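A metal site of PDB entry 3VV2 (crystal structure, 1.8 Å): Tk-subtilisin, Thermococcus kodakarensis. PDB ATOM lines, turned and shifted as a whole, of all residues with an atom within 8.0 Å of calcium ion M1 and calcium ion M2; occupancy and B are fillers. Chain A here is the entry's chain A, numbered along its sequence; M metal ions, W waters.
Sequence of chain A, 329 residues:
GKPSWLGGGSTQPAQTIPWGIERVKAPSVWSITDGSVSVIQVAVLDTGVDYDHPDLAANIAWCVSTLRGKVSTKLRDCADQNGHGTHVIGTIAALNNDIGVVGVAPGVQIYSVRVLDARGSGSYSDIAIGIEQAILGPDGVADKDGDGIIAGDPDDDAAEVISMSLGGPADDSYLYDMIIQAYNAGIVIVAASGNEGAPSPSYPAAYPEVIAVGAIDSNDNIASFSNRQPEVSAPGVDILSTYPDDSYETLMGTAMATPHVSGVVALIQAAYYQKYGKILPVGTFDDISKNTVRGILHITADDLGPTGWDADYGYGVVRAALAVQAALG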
ATOM      1  N   VAL A 141      23.626  -2.406 -21.285  1.00  0.00           N
ATOM      2  CA  VAL A 141      23.924  -3.103 -22.527  1.00  0.00           C
ATOM      3  C   VAL A 141      23.953  -4.631 -22.239  1.00  0.00           C
ATOM      4  O   VAL A 141      24.635  -5.086 -21.304  1.00  0.00           O
ATOM      5  CB  VAL A 141      25.280  -2.595 -23.149  1.00  0.00           C
ATOM      6  CG1 VAL A 141      25.552  -3.226 -24.539  1.00  0.00           C
ATOM      7  CG2 VAL A 141      25.318  -1.033 -23.198  1.00  0.00           C
ATOM      8  N   ALA A 142      23.184  -5.364 -23.026  1.00  0.00           N
ATOM      9  CA  ALA A 142      23.065  -6.795 -22.904  1.00  0.00           C
ATOM     10  C   ALA A 142      24.412  -7.476 -23.208  1.00  0.00           C
ATOM     11  O   ALA A 142      24.998  -8.130 -22.318  1.00  0.00           O
ATOM     12  CB  ALA A 142      21.991  -7.262 -23.860  1.00  0.00           C
ATOM     13  N   ASP A 143      24.968  -7.197 -24.398  1.00  0.00           N
ATOM     14  CA  ASP A 143      26.159  -7.898 -24.901  1.00  0.00           C
ATOM     15  C   ASP A 143      27.194  -6.888 -25.423  1.00  0.00           C
ATOM     16  O   ASP A 143      27.234  -6.624 -26.657  1.00  0.00           O
ATOM     17  CB  ASP A 143      25.699  -8.819 -26.050  1.00  0.00           C
ATOM     18  CG  ASP A 143      26.854  -9.652 -26.658  1.00  0.00           C
ATOM     19  OD1 ASP A 143      27.924  -9.700 -26.084  1.00  0.00           O
ATOM     20  OD2 ASP A 143      26.650 -10.315 -27.656  1.00  0.00           O
ATOM     21  N   LYS A 144      28.023  -6.336 -24.534  1.00  0.00           N
ATOM     22  CA  LYS A 144      28.858  -5.180 -24.871  1.00  0.00           C
ATOM     23  C   LYS A 144      29.924  -5.492 -25.942  1.00  0.00           C
ATOM     24  O   LYS A 144      30.217  -4.636 -26.790  1.00  0.00           O
ATOM     25  CB  LYS A 144      29.616  -4.754 -23.633  1.00  0.00           C
ATOM     26  CG  LYS A 144      29.336  -3.358 -23.208  1.00  0.00           C
ATOM     27  CD  LYS A 144      29.925  -3.153 -21.808  1.00  0.00           C
ATOM     28  CE  LYS A 144      31.438  -3.346 -21.798  1.00  0.00           C
ATOM     29  NZ  LYS A 144      31.852  -3.959 -20.505  1.00  0.00           N
ATOM     30  N   ASP A 145      30.459  -6.699 -25.936  1.00  0.00           N
ATOM     31  CA  ASP A 145      31.471  -7.059 -26.886  1.00  0.00           C
ATOM     32  C   ASP A 145      30.959  -7.801 -28.122  1.00  0.00           C
ATOM     33  O   ASP A 145      31.719  -8.136 -28.996  1.00  0.00           O
ATOM     34  CB  ASP A 145      32.607  -7.793 -26.208  1.00  0.00           C
ATOM     35  CG  ASP A 145      32.174  -9.101 -25.594  1.00  0.00           C
ATOM     36  OD1 ASP A 145      33.033  -9.766 -24.997  1.00  0.00           O
ATOM     37  OD2 ASP A 145      31.025  -9.546 -25.654  1.00  0.00           O
ATOM     38  N   GLY A 146      29.661  -8.032 -28.197  1.00  0.00           N
ATOM     39  CA  GLY A 146      29.047  -8.555 -29.432  1.00  0.00           C
ATOM     40  C   GLY A 146      29.298  -9.999 -29.734  1.00  0.00           C
ATOM     41  O   GLY A 146      29.028 -10.487 -30.877  1.00  0.00           O
ATOM     42  N   ASP A 147      29.799 -10.721 -28.750  1.00  0.00           N
ATOM     43  CA  ASP A 147      30.105 -12.164 -28.982  1.00  0.00           C
ATOM     44  C   ASP A 147      28.963 -13.166 -28.767  1.00  0.00           C
ATOM     45  O   ASP A 147      29.157 -14.359 -29.015  1.00  0.00           O
ATOM     46  CB  ASP A 147      31.346 -12.635 -28.225  1.00  0.00           C
ATOM     47  CG  ASP A 147      31.208 -12.462 -26.691  1.00  0.00           C
ATOM     48  OD1 ASP A 147      30.107 -12.219 -26.105  1.00  0.00           O
ATOM     49  OD2 ASP A 147      32.245 -12.535 -26.060  1.00  0.00           O
ATOM     50  N   GLY A 148      27.788 -12.709 -28.376  1.00  0.00           N
ATOM     51  CA  GLY A 148      26.638 -13.655 -28.178  1.00  0.00           C
ATOM     52  C   GLY A 148      26.645 -14.306 -26.804  1.00  0.00           C
ATOM     53  O   GLY A 148      25.751 -14.996 -26.416  1.00  0.00           O
ATOM     54  N   ILE A 149      27.707 -14.094 -26.018  1.00  0.00           N
ATOM     55  CA  ILE A 149      27.747 -14.666 -24.701  1.00  0.00           C
ATOM     56  C   ILE A 149      27.264 -13.531 -23.780  1.00  0.00           C
ATOM     57  O   ILE A 149      27.809 -12.457 -23.851  1.00  0.00           O
ATOM     58  CB  ILE A 149      29.213 -15.067 -24.316  1.00  0.00           C
ATOM     59  CG1 ILE A 149      29.958 -15.727 -25.518  1.00  0.00           C
ATOM     60  CG2 ILE A 149      29.245 -15.915 -23.015  1.00  0.00           C
ATOM     61  CD1 ILE A 149      31.138 -16.622 -25.122  1.00  0.00           C
ATOM     62  N   ILE A 150      26.259 -13.776 -22.985  1.00  0.00           N
ATOM     63  CA  ILE A 150      25.753 -12.786 -22.067  1.00  0.00           C
ATOM     64  C   ILE A 150      25.860 -13.297 -20.622  1.00  0.00           C
ATOM     65  O   ILE A 150      26.685 -12.848 -19.881  1.00  0.00           O
ATOM     66  CB  ILE A 150      24.331 -12.317 -22.446  1.00  0.00           C
ATOM     67  CG1 ILE A 150      24.327 -11.658 -23.815  1.00  0.00           C
ATOM     68  CG2 ILE A 150      23.809 -11.328 -21.426  1.00  0.00           C
ATOM     69  CD1 ILE A 150      23.079 -11.807 -24.531  1.00  0.00           C
ATOM     70  N   ALA A 151      25.077 -14.285 -20.241  1.00  0.00           N
ATOM     71  CA  ALA A 151      25.198 -14.792 -18.885  1.00  0.00           C
ATOM     72  C   ALA A 151      26.506 -15.561 -19.041  1.00  0.00           C
ATOM     73  O   ALA A 151      26.756 -16.181 -20.103  1.00  0.00           O
ATOM     74  CB  ALA A 151      24.014 -15.757 -18.566  1.00  0.00           C
ATOM     75  N   GLY A 152      27.346 -15.485 -18.012  1.00  0.00           N
ATOM     76  CA  GLY A 152      28.662 -16.147 -18.028  1.00  0.00           C
ATOM     77  C   GLY A 152      29.816 -15.469 -18.753  1.00  0.00           C
ATOM     78  O   GLY A 152      30.972 -15.951 -18.695  1.00  0.00           O
ATOM     79  N   ASP A 153      29.545 -14.376 -19.451  1.00  0.00           N
ATOM     80  CA  ASP A 153      30.608 -13.568 -20.022  1.00  0.00           C
ATOM     81  C   ASP A 153      31.175 -12.628 -18.988  1.00  0.00           C
ATOM     82  O   ASP A 153      30.484 -11.747 -18.511  1.00  0.00           O
ATOM     83  CB  ASP A 153      30.103 -12.798 -21.235  1.00  0.00           C
ATOM     84  CG  ASP A 153      31.216 -12.129 -22.013  1.00  0.00           C
ATOM     85  OD1 ASP A 153      30.986 -11.755 -23.169  1.00  0.00           O
ATOM     86  OD2 ASP A 153      32.336 -11.942 -21.540  1.00  0.00           O
ATOM     87  N   PRO A 154      32.429 -12.811 -18.602  1.00  0.00           N
ATOM     88  CA  PRO A 154      32.927 -11.868 -17.582  1.00  0.00           C
ATOM     89  C   PRO A 154      33.019 -10.396 -17.998  1.00  0.00           C
ATOM     90  O   PRO A 154      33.127  -9.551 -17.099  1.00  0.00           O
ATOM     91  CB  PRO A 154      34.305 -12.405 -17.208  1.00  0.00           C
ATOM     92  CG  PRO A 154      34.724 -13.304 -18.396  1.00  0.00           C
ATOM     93  CD  PRO A 154      33.456 -13.776 -19.071  1.00  0.00           C
ATOM     94  N   ASP A 155      32.966 -10.116 -19.304  1.00  0.00           N
ATOM     95  CA  ASP A 155      33.013  -8.733 -19.861  1.00  0.00           C
ATOM     96  C   ASP A 155      31.618  -8.083 -19.722  1.00  0.00           C
ATOM     97  O   ASP A 155      31.459  -6.828 -19.674  1.00  0.00           O
ATOM     98  CB  ASP A 155      33.483  -8.683 -21.338  1.00  0.00           C
ATOM     99  CG  ASP A 155      33.602  -7.276 -21.829  1.00  0.00           C
ATOM    100  OD1 ASP A 155      34.293  -6.499 -21.143  1.00  0.00           O
ATOM    101  OD2 ASP A 155      32.963  -6.875 -22.827  1.00  0.00           O
ATOM    102  N   ASP A 156      30.603  -8.916 -19.605  1.00  0.00           N
ATOM    103  CA  ASP A 156      29.272  -8.350 -19.318  1.00  0.00           C
ATOM    104  C   ASP A 156      28.852  -8.388 -17.818  1.00  0.00           C
ATOM    105  O   ASP A 156      29.535  -8.973 -16.978  1.00  0.00           O
ATOM    106  CB  ASP A 156      28.192  -9.004 -20.175  1.00  0.00           C
ATOM    107  CG  ASP A 156      28.316  -8.647 -21.667  1.00  0.00           C
ATOM    108  OD1 ASP A 156      28.313  -7.441 -21.984  1.00  0.00           O
ATOM    109  OD2 ASP A 156      28.405  -9.562 -22.507  1.00  0.00           O
ATOM    110  N   ASP A 157      27.731  -7.759 -17.518  1.00  0.00           N
ATOM    111  CA  ASP A 157      27.227  -7.703 -16.149  1.00  0.00           C
ATOM    112  C   ASP A 157      25.813  -8.238 -16.056  1.00  0.00           C
ATOM    113  O   ASP A 157      25.063  -7.876 -15.151  1.00  0.00           O
ATOM    114  CB  ASP A 157      27.290  -6.267 -15.619  1.00  0.00           C
ATOM    115  CG  ASP A 157      26.570  -5.282 -16.513  1.00  0.00           C
ATOM    116  OD1 ASP A 157      26.626  -4.067 -16.222  1.00  0.00           O
ATOM    117  OD2 ASP A 157      25.961  -5.717 -17.507  1.00  0.00           O
HETATM  118 CA    CA M   1      32.730 -11.665 -24.324  1.00  0.00          CA
HETATM  119 CA    CA M   2      29.373 -10.638 -24.448  1.00  0.00          CA
HETATM  120  O   HOH W   1      30.589  -8.405 -23.289  1.00  0.00           O
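Of the 17 residues printed, 3 come within 4 Å of calcium ion M1.
The nearest printed residue that does not touch calcium ion M1 is Asp 155 (4.3 Å).
Water W1 lies within hydrogen-bond range of OD1 of Asp 156, OD2 of Asp 155 and N of Asp 145.
Within 4 Å of calcium ion M2: Asp 143, Asp 145, Asp 147, Ile 149, Asp 153 and Asp 156.
The nearest printed residue that does not touch calcium ion M2 is Lys 144 (4.5 Å).
Calcium ion M2 is bound by OD2 of Asp 145 (2.3 Å), OD1 of Asp 153 (2.3 Å), OD1 of Asp 143 (2.4 Å), OD1 of Asp 147 (2.4 Å), OD2 of Asp 156 (2.4 Å), O of Ile 149 (2.5 Å) and water W1 (2.8 Å).
Calcium ion M2 has seven donor atoms within binding distance.
The side-chain carboxylate of Asp 153 lies close to the backbone NH of Asp 155.
The side-chain carboxylate of Asp 143 lies close to the backbone NH of Gly 146 (3.2 Å).
OD2 of Asp 143 lies within hydrogen-bond range of N of Gly 148, at 2.7 Å.
The side-chain carboxylate of Asp 156 lies within hydrogen-bond range of the backbone NH of Lys 144 (2.8 Å).
Calcium ion M1 is bound by OD2 of Asp 147 (2.0 Å), OD1 of Asp 145 (2.0 Å), OD1 of Asp 153 (2.1 Å) and OD2 of Asp 153 (2.8 Å).
Calcium ion M1 has four donor atoms within binding distance.
Slightly farther from calcium ion M1 lies OD2 of Asp 145 (3.0 Å).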
